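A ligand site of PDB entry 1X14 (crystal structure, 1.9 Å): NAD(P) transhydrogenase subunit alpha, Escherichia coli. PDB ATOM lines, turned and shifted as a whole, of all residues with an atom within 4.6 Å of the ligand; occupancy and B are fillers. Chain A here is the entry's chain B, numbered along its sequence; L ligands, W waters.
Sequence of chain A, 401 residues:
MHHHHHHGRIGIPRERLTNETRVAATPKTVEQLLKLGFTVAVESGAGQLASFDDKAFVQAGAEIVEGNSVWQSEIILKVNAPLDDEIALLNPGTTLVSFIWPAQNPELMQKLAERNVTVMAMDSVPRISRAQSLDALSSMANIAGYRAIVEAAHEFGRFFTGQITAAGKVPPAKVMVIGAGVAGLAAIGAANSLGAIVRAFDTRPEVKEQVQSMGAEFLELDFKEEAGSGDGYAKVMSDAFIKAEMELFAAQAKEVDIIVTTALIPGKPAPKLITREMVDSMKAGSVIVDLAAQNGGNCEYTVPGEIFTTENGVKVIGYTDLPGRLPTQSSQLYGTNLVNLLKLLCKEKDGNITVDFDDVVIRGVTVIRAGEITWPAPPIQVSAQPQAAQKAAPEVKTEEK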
ATOM      1  N   ARG A 127     -14.846 -25.426  17.317  1.00  0.00           N
ATOM      2  CA  ARG A 127     -14.140 -24.507  16.408  1.00  0.00           C
ATOM      3  C   ARG A 127     -12.631 -24.551  16.655  1.00  0.00           C
ATOM      4  O   ARG A 127     -12.024 -23.566  17.075  1.00  0.00           O
ATOM      5  CB  ARG A 127     -14.710 -23.089  16.513  1.00  0.00           C
ATOM      6  CG  ARG A 127     -16.268 -23.008  16.407  1.00  0.00           C
ATOM      7  CD  ARG A 127     -16.919 -23.605  15.138  1.00  0.00           C
ATOM      8  NE  ARG A 127     -18.012 -22.769  14.585  1.00  0.00           N
ATOM      9  CZ  ARG A 127     -17.854 -21.755  13.694  1.00  0.00           C
ATOM     10  NH1 ARG A 127     -16.651 -21.430  13.209  1.00  0.00           N
ATOM     11  NH2 ARG A 127     -18.906 -21.030  13.312  1.00  0.00           N
ATOM     12  N   ILE A 128     -12.027 -25.712  16.428  1.00  0.00           N
ATOM     13  CA  ILE A 128     -10.575 -25.791  16.400  1.00  0.00           C
ATOM     14  C   ILE A 128     -10.091 -25.887  14.996  1.00  0.00           C
ATOM     15  O   ILE A 128     -10.834 -26.222  14.072  1.00  0.00           O
ATOM     16  CB  ILE A 128     -10.048 -26.960  17.265  1.00  0.00           C
ATOM     17  CG1 ILE A 128     -10.534 -28.311  16.768  1.00  0.00           C
ATOM     18  CG2 ILE A 128     -10.442 -26.744  18.698  1.00  0.00           C
ATOM     19  CD1 ILE A 128      -9.742 -29.477  17.371  1.00  0.00           C
ATOM     20  N   SER A 129      -8.804 -25.605  14.805  1.00  0.00           N
ATOM     21  CA  SER A 129      -8.277 -25.451  13.457  1.00  0.00           C
ATOM     22  C   SER A 129      -8.357 -26.744  12.659  1.00  0.00           C
ATOM     23  O   SER A 129      -8.606 -26.712  11.443  1.00  0.00           O
ATOM     24  CB  SER A 129      -6.812 -24.961  13.526  1.00  0.00           C
ATOM     25  OG  SER A 129      -6.818 -23.579  13.776  1.00  0.00           O
ATOM     26  N   GLN A 132     -11.690 -27.362  10.786  1.00  0.00           N
ATOM     27  CA  GLN A 132     -12.168 -26.414   9.776  1.00  0.00           C
ATOM     28  C   GLN A 132     -12.732 -27.067   8.534  1.00  0.00           C
ATOM     29  O   GLN A 132     -13.617 -26.516   7.902  1.00  0.00           O
ATOM     30  CB  GLN A 132     -11.080 -25.395   9.403  1.00  0.00           C
ATOM     31  CG  GLN A 132     -11.094 -24.211  10.350  1.00  0.00           C
ATOM     32  CD  GLN A 132     -12.510 -23.886  10.861  1.00  0.00           C
ATOM     33  OE1 GLN A 132     -12.861 -24.218  12.016  1.00  0.00           O
ATOM     34  NE2 GLN A 132     -13.310 -23.261   9.993  1.00  0.00           N
ATOM     35  N   SER A 138     -18.900 -22.170   9.266  1.00  0.00           N
ATOM     36  CA  SER A 138     -18.017 -21.368   8.476  1.00  0.00           C
ATOM     37  C   SER A 138     -18.410 -21.431   6.981  1.00  0.00           C
ATOM     38  O   SER A 138     -18.474 -20.417   6.304  1.00  0.00           O
ATOM     39  CB  SER A 138     -16.566 -21.798   8.654  1.00  0.00           C
ATOM     40  OG  SER A 138     -16.178 -21.609  10.017  1.00  0.00           O
ATOM     41  N   ILE A 178     -19.442  -4.434   8.598  1.00  0.00           N
ATOM     42  CA  ILE A 178     -19.454  -4.590  10.064  1.00  0.00           C
ATOM     43  C   ILE A 178     -19.337  -6.043  10.522  1.00  0.00           C
ATOM     44  O   ILE A 178     -20.240  -6.872  10.349  1.00  0.00           O
ATOM     45  CB  ILE A 178     -20.694  -3.928  10.673  1.00  0.00           C
ATOM     46  CG1 ILE A 178     -20.662  -2.424  10.333  1.00  0.00           C
ATOM     47  CG2 ILE A 178     -20.706  -4.079  12.185  1.00  0.00           C
ATOM     48  CD1 ILE A 178     -21.953  -1.669  10.630  1.00  0.00           C
ATOM     49  N   GLY A 179     -18.194  -6.366  11.088  1.00  0.00           N
ATOM     50  CA  GLY A 179     -17.887  -7.692  11.519  1.00  0.00           C
ATOM     51  C   GLY A 179     -17.086  -8.274  10.408  1.00  0.00           C
ATOM     52  O   GLY A 179     -17.566  -8.324   9.288  1.00  0.00           O
ATOM     53  N   ALA A 180     -15.872  -8.668  10.725  1.00  0.00           N
ATOM     54  CA  ALA A 180     -14.926  -9.217   9.792  1.00  0.00           C
ATOM     55  C   ALA A 180     -14.566 -10.614  10.232  1.00  0.00           C
ATOM     56  O   ALA A 180     -13.404 -11.015  10.205  1.00  0.00           O
ATOM     57  CB  ALA A 180     -13.701  -8.347   9.757  1.00  0.00           C
ATOM     58  N   GLY A 181     -15.574 -11.366  10.670  1.00  0.00           N
ATOM     59  CA  GLY A 181     -15.474 -12.803  10.748  1.00  0.00           C
ATOM     60  C   GLY A 181     -15.581 -13.474   9.365  1.00  0.00           C
ATOM     61  O   GLY A 181     -15.247 -12.901   8.328  1.00  0.00           O
ATOM     62  N   VAL A 182     -16.038 -14.715   9.345  1.00  0.00           N
ATOM     63  CA  VAL A 182     -16.026 -15.467   8.096  1.00  0.00           C
ATOM     64  C   VAL A 182     -16.900 -14.807   7.037  1.00  0.00           C
ATOM     65  O   VAL A 182     -16.480 -14.697   5.890  1.00  0.00           O
ATOM     66  CB  VAL A 182     -16.412 -16.923   8.317  1.00  0.00           C
ATOM     67  CG1 VAL A 182     -16.392 -17.703   6.966  1.00  0.00           C
ATOM     68  CG2 VAL A 182     -15.458 -17.559   9.315  1.00  0.00           C
ATOM     69  N   PHE A 201     -15.065  -2.785  10.092  1.00  0.00           N
ATOM     70  CA  PHE A 201     -14.829  -2.768  11.511  1.00  0.00           C
ATOM     71  C   PHE A 201     -15.151  -4.105  12.202  1.00  0.00           C
ATOM     72  O   PHE A 201     -16.097  -4.799  11.828  1.00  0.00           O
ATOM     73  CB  PHE A 201     -15.617  -1.661  12.157  1.00  0.00           C
ATOM     74  CG  PHE A 201     -15.303  -1.495  13.594  1.00  0.00           C
ATOM     75  CD1 PHE A 201     -14.224  -0.723  13.986  1.00  0.00           C
ATOM     76  CD2 PHE A 201     -16.071  -2.147  14.563  1.00  0.00           C
ATOM     77  CE1 PHE A 201     -13.914  -0.578  15.317  1.00  0.00           C
ATOM     78  CE2 PHE A 201     -15.756  -2.023  15.915  1.00  0.00           C
ATOM     79  CZ  PHE A 201     -14.691  -1.231  16.282  1.00  0.00           C
ATOM     80  N   ASP A 202     -14.323  -4.468  13.178  1.00  0.00           N
ATOM     81  CA  ASP A 202     -14.514  -5.582  14.080  1.00  0.00           C
ATOM     82  C   ASP A 202     -13.949  -5.192  15.470  1.00  0.00           C
ATOM     83  O   ASP A 202     -12.977  -4.462  15.553  1.00  0.00           O
ATOM     84  CB  ASP A 202     -13.767  -6.813  13.546  1.00  0.00           C
ATOM     85  CG  ASP A 202     -14.307  -8.143  14.102  1.00  0.00           C
ATOM     86  OD1 ASP A 202     -14.132  -8.459  15.318  1.00  0.00           O
ATOM     87  OD2 ASP A 202     -14.927  -8.955  13.379  1.00  0.00           O
ATOM     88  N   THR A 203     -14.531  -5.699  16.536  1.00  0.00           N
ATOM     89  CA  THR A 203     -14.000  -5.435  17.875  1.00  0.00           C
ATOM     90  C   THR A 203     -12.711  -6.209  18.148  1.00  0.00           C
ATOM     91  O   THR A 203     -11.926  -5.807  19.004  1.00  0.00           O
ATOM     92  CB  THR A 203     -15.046  -5.774  18.920  1.00  0.00           C
ATOM     93  OG1 THR A 203     -15.564  -7.065  18.664  1.00  0.00           O
ATOM     94  CG2 THR A 203     -16.261  -4.874  18.780  1.00  0.00           C
ATOM     95  N   ARG A 204     -12.468  -7.294  17.418  1.00  0.00           N
ATOM     96  CA  ARG A 204     -11.304  -8.119  17.617  1.00  0.00           C
ATOM     97  C   ARG A 204     -10.158  -7.561  16.757  1.00  0.00           C
ATOM     98  O   ARG A 204     -10.137  -7.770  15.554  1.00  0.00           O
ATOM     99  CB  ARG A 204     -11.557  -9.589  17.262  1.00  0.00           C
ATOM    100  CG  ARG A 204     -12.782 -10.243  17.893  1.00  0.00           C
ATOM    101  CD  ARG A 204     -12.928 -11.754  17.564  1.00  0.00           C
ATOM    102  NE  ARG A 204     -13.396 -12.021  16.185  1.00  0.00           N
ATOM    103  CZ  ARG A 204     -12.631 -12.467  15.173  1.00  0.00           C
ATOM    104  NH1 ARG A 204     -11.321 -12.687  15.312  1.00  0.00           N
ATOM    105  NH2 ARG A 204     -13.186 -12.681  13.989  1.00  0.00           N
ATOM    106  N   GLU A 245     -18.294   3.172  19.157  1.00  0.00           N
ATOM    107  CA  GLU A 245     -18.593   2.312  17.997  1.00  0.00           C
ATOM    108  C   GLU A 245     -19.798   2.817  17.231  1.00  0.00           C
ATOM    109  O   GLU A 245     -19.798   2.780  16.009  1.00  0.00           O
ATOM    110  CB  GLU A 245     -18.796   0.845  18.404  1.00  0.00           C
ATOM    111  CG  GLU A 245     -19.136  -0.063  17.229  1.00  0.00           C
ATOM    112  CD  GLU A 245     -19.154  -1.518  17.618  1.00  0.00           C
ATOM    113  OE1 GLU A 245     -18.418  -2.309  16.990  1.00  0.00           O
ATOM    114  OE2 GLU A 245     -19.895  -1.870  18.536  1.00  0.00           O
ATOM    115  N   PHE A 249     -20.152   4.333  13.316  1.00  0.00           N
ATOM    116  CA  PHE A 249     -21.108   3.848  12.304  1.00  0.00           C
ATOM    117  C   PHE A 249     -22.012   4.985  11.836  1.00  0.00           C
ATOM    118  O   PHE A 249     -22.318   5.051  10.658  1.00  0.00           O
ATOM    119  CB  PHE A 249     -21.887   2.636  12.804  1.00  0.00           C
ATOM    120  CG  PHE A 249     -21.027   1.452  13.145  1.00  0.00           C
ATOM    121  CD1 PHE A 249     -21.496   0.488  13.992  1.00  0.00           C
ATOM    122  CD2 PHE A 249     -19.748   1.304  12.622  1.00  0.00           C
ATOM    123  CE1 PHE A 249     -20.709  -0.599  14.332  1.00  0.00           C
ATOM    124  CE2 PHE A 249     -18.962   0.226  12.963  1.00  0.00           C
ATOM    125  CZ  PHE A 249     -19.455  -0.733  13.812  1.00  0.00           C
ATOM    126  N   THR A 262     -22.721  -8.227   9.830  1.00  0.00           N
ATOM    127  CA  THR A 262     -22.591  -9.653  10.056  1.00  0.00           C
ATOM    128  C   THR A 262     -22.413 -10.025  11.527  1.00  0.00           C
ATOM    129  O   THR A 262     -21.982 -11.146  11.831  1.00  0.00           O
ATOM    130  CB  THR A 262     -21.360 -10.151   9.332  1.00  0.00           C
ATOM    131  OG1 THR A 262     -20.198  -9.623   9.976  1.00  0.00           O
ATOM    132  CG2 THR A 262     -21.297  -9.625   7.884  1.00  0.00           C
ATOM    133  N   ALA A 263     -22.715  -9.105  12.421  1.00  0.00           N
ATOM    134  CA  ALA A 263     -22.275  -9.226  13.811  1.00  0.00           C
ATOM    135  C   ALA A 263     -23.209 -10.054  14.652  1.00  0.00           C
ATOM    136  O   ALA A 263     -24.389  -9.734  14.821  1.00  0.00           O
ATOM    137  CB  ALA A 263     -22.101  -7.865  14.453  1.00  0.00           C
ATOM    138  N   LEU A 264     -22.653 -11.148  15.158  1.00  0.00           N
ATOM    139  CA  LEU A 264     -23.315 -11.956  16.174  1.00  0.00           C
ATOM    140  C   LEU A 264     -22.340 -12.150  17.324  1.00  0.00           C
ATOM    141  O   LEU A 264     -21.110 -12.106  17.127  1.00  0.00           O
ATOM    142  CB  LEU A 264     -23.715 -13.320  15.589  1.00  0.00           C
ATOM    143  CG  LEU A 264     -24.507 -13.193  14.283  1.00  0.00           C
ATOM    144  CD1 LEU A 264     -24.135 -14.247  13.238  1.00  0.00           C
ATOM    145  CD2 LEU A 264     -25.965 -13.239  14.615  1.00  0.00           C
ATOM    146  N   ILE A 265     -22.901 -12.337  18.517  1.00  0.00           N
ATOM    147  CA  ILE A 265     -22.162 -12.762  19.708  1.00  0.00           C
ATOM    148  C   ILE A 265     -22.754 -14.109  20.118  1.00  0.00           C
ATOM    149  O   ILE A 265     -23.977 -14.203  20.318  1.00  0.00           O
ATOM    150  CB  ILE A 265     -22.333 -11.761  20.895  1.00  0.00           C
ATOM    151  CG1 ILE A 265     -22.187 -10.300  20.418  1.00  0.00           C
ATOM    152  CG2 ILE A 265     -21.353 -12.120  22.047  1.00  0.00           C
ATOM    153  CD1 ILE A 265     -21.605  -9.326  21.478  1.00  0.00           C
ATOM    154  N   PRO A 266     -21.922 -15.143  20.244  1.00  0.00           N
ATOM    155  CA  PRO A 266     -22.441 -16.482  20.542  1.00  0.00           C
ATOM    156  C   PRO A 266     -23.321 -16.521  21.817  1.00  0.00           C
ATOM    157  O   PRO A 266     -22.840 -16.179  22.896  1.00  0.00           O
ATOM    158  CB  PRO A 266     -21.166 -17.341  20.705  1.00  0.00           C
ATOM    159  CG  PRO A 266     -20.016 -16.391  20.830  1.00  0.00           C
ATOM    160  CD  PRO A 266     -20.443 -15.127  20.148  1.00  0.00           C
ATOM    161  N   LEU A 273     -26.698  -2.355  15.876  1.00  0.00           N
ATOM    162  CA  LEU A 273     -25.546  -1.526  15.581  1.00  0.00           C
ATOM    163  C   LEU A 273     -25.857  -0.371  14.616  1.00  0.00           C
ATOM    164  O   LEU A 273     -25.171   0.663  14.627  1.00  0.00           O
ATOM    165  CB  LEU A 273     -24.430  -2.404  15.008  1.00  0.00           C
ATOM    166  CG  LEU A 273     -23.918  -3.446  16.003  1.00  0.00           C
ATOM    167  CD1 LEU A 273     -22.727  -4.206  15.442  1.00  0.00           C
ATOM    168  CD2 LEU A 273     -23.533  -2.792  17.346  1.00  0.00           C
HETATM  169  P1  LIG L   1     -19.347 -14.584  14.215  1.00  0.00           P
HETATM  170  O1  LIG L   1     -20.132 -15.125  13.122  1.00  0.00           O
HETATM  171  O2  LIG L   1     -19.920 -14.907  15.608  1.00  0.00           O
HETATM  172  O3  LIG L   1     -19.549 -12.980  14.105  1.00  0.00           O
HETATM  173  C1  LIG L   1     -18.969 -12.238  13.051  1.00  0.00           C
HETATM  174  C2  LIG L   1     -18.094 -11.116  13.613  1.00  0.00           C
HETATM  175  O4  LIG L   1     -18.888 -10.146  14.274  1.00  0.00           O
HETATM  176  C3  LIG L   1     -16.997 -11.575  14.597  1.00  0.00           C
HETATM  177  O5  LIG L   1     -15.705 -11.417  14.029  1.00  0.00           O
HETATM  178  C4  LIG L   1     -17.243 -10.708  15.824  1.00  0.00           C
HETATM  179  O6  LIG L   1     -16.131 -10.285  16.569  1.00  0.00           O
HETATM  180  C5  LIG L   1     -17.954  -9.561  15.175  1.00  0.00           C
HETATM  181  N1  LIG L   1     -18.662  -8.703  16.104  1.00  0.00           N
HETATM  182  C6  LIG L   1     -19.403  -9.043  17.212  1.00  0.00           C
HETATM  183  N2  LIG L   1     -19.870  -7.874  17.743  1.00  0.00           N
HETATM  184  C7  LIG L   1     -19.417  -6.821  16.995  1.00  0.00           C
HETATM  185  C8  LIG L   1     -19.556  -5.442  17.099  1.00  0.00           C
HETATM  186  N3  LIG L   1     -20.290  -4.934  18.070  1.00  0.00           N
HETATM  187  N4  LIG L   1     -18.988  -4.612  16.158  1.00  0.00           N
HETATM  188  C9  LIG L   1     -18.200  -5.165  15.135  1.00  0.00           C
HETATM  189  N5  LIG L   1     -18.022  -6.528  15.062  1.00  0.00           N
HETATM  190  C10 LIG L   1     -18.641  -7.345  15.962  1.00  0.00           C
HETATM  191  O7  LIG L   1     -17.737 -14.902  14.152  1.00  0.00           O
HETATM  192  P2  LIG L   1     -16.794 -15.830  13.199  1.00  0.00           P
HETATM  193  O8  LIG L   1     -15.367 -15.385  13.320  1.00  0.00           O
HETATM  194  O9  LIG L   1     -17.361 -15.812  11.834  1.00  0.00           O
HETATM  195  O10 LIG L   1     -16.766 -17.344  13.849  1.00  0.00           O
HETATM  196  C11 LIG L   1     -17.081 -17.639  15.225  1.00  0.00           C
HETATM  197  C12 LIG L   1     -16.137 -18.628  15.939  1.00  0.00           C
HETATM  198  O11 LIG L   1     -15.659 -19.657  15.066  1.00  0.00           O
HETATM  199  C13 LIG L   1     -14.892 -17.965  16.546  1.00  0.00           C
HETATM  200  O12 LIG L   1     -14.600 -18.440  17.857  1.00  0.00           O
HETATM  201  C14 LIG L   1     -13.780 -18.353  15.605  1.00  0.00           C
HETATM  202  O13 LIG L   1     -12.501 -18.414  16.214  1.00  0.00           O
HETATM  203  C15 LIG L   1     -14.224 -19.714  15.091  1.00  0.00           C
HETATM  204  N6  LIG L   1     -13.530 -19.951  13.793  1.00  0.00           N
HETATM  205  C16 LIG L   1     -12.298 -20.551  13.856  1.00  0.00           C
HETATM  206  C17 LIG L   1     -11.548 -20.790  12.702  1.00  0.00           C
HETATM  207  C18 LIG L   1     -10.192 -21.469  12.791  1.00  0.00           C
HETATM  208  O14 LIG L   1      -9.465 -21.711  11.616  1.00  0.00           O
HETATM  209  N7  LIG L   1      -9.702 -21.846  13.975  1.00  0.00           N
HETATM  210  C19 LIG L   1     -12.072 -20.395  11.464  1.00  0.00           C
HETATM  211  C20 LIG L   1     -13.316 -19.779  11.421  1.00  0.00           C
HETATM  212  C21 LIG L   1     -14.035 -19.554  12.585  1.00  0.00           C
HETATM  213  O   HOH W   1     -19.139 -14.605  10.234  1.00  0.00           O
HETATM  214  O   HOH W   2     -18.168 -11.824   9.895  1.00  0.00           O
HETATM  215  O   HOH W   3     -13.341 -16.352  12.157  1.00  0.00           O
HETATM  216  O   HOH W   4     -18.801 -13.143  18.114  1.00  0.00           O
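NH2 of Arg 204 is in salt-bridge range of O8 of the ligand (3.5 Å).
O5 of the ligand sits at hydrogen-bond distance from OD2 of Asp 202.
The guanidinium group (NH1) of Arg 127 is in hydrogen-bond range of an oxygen (O11) of the ligand (2.8 Å).
N of Gly 181 sits at hydrogen-bond distance from O5 of the ligand (3.4 Å).
N of Val 182 lies within hydrogen-bond range of O9 of the ligand (3.0 Å).
The side-chain hydroxyl (OG) of Ser 129 is in hydrogen-bond range of a nitrogen (N7) of the ligand, 3.4 Å away.
The side-chain carboxylate (OE1) of Glu 245 lies within hydrogen-bond range of a nitrogen (N4) of the ligand (2.5 Å).
The backbone carbonyl oxygen (O) of Ile 178 lies within hydrogen-bond range of the side-chain hydroxyl (OG1) of Thr 262 (2.8 Å).
The side-chain hydroxyl of Ser 138 sits at hydrogen-bond distance from the side-chain amide nitrogen of Gln 132, at 3.3 Å.
OG1 of Thr 262 sits at hydrogen-bond distance from O of Gly 179 (3.0 Å).
The backbone carbonyl oxygen of Phe 201 sits at hydrogen-bond distance from the backbone NH of Gly 179.
OD1 of Asp 202 lies within salt-bridge range of NE of Arg 204 (3.7 Å).
The guanidinium group (NH1) of Arg 127 lies within hydrogen-bond range of the side-chain hydroxyl (OG) of Ser 138 (3.2 Å).
The side-chain carboxylate (OD2) of Asp 202 lies within hydrogen-bond range of the backbone NH (N) of Ala 180, 2.8 Å away.
An oxygen (O2) of the ligand sits close to the backbone carbonyl oxygen of Leu 264 (3.4 Å).
Gln 132 touches the ligand (CG to O14, 3.2 Å).
Ser 138 touches the ligand (OG to C20, 3.7 Å).
CA of Gly 179 touches N5 of the ligand, 3.7 Å away.
Phe 201 touches the ligand (CD2 to C9, 3.7 Å).
CG2 of Thr 203 touches C8 of the ligand, at 3.7 Å.
Thr 262 touches the ligand (O to C1, 3.4 Å).
Ala 263 touches the ligand.
CD1 of Leu 273 touches N3 of the ligand, 3.7 Å away.
Hydrophobic or aromatic side chains that line the ligand: Val 182, Phe 201, Ala 263 and Leu 273.
The nearest printed residue that does not touch the ligand is Ile 178 (4.02 Å).
Water W1 lies within hydrogen-bond range of an oxygen (O9) of the ligand (2.7 Å) and the backbone NH of Val 182 (3.2 Å).
Water W4 lies within hydrogen-bond range of the backbone carbonyl oxygen of Leu 264 (2.7 Å) and an oxygen (O2) of the ligand (3.3 Å).
Water W2 lies within hydrogen-bond range of the backbone NH of Gly 181 (2.7 Å) and the side-chain hydroxyl of Thr 262 (3.0 Å).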
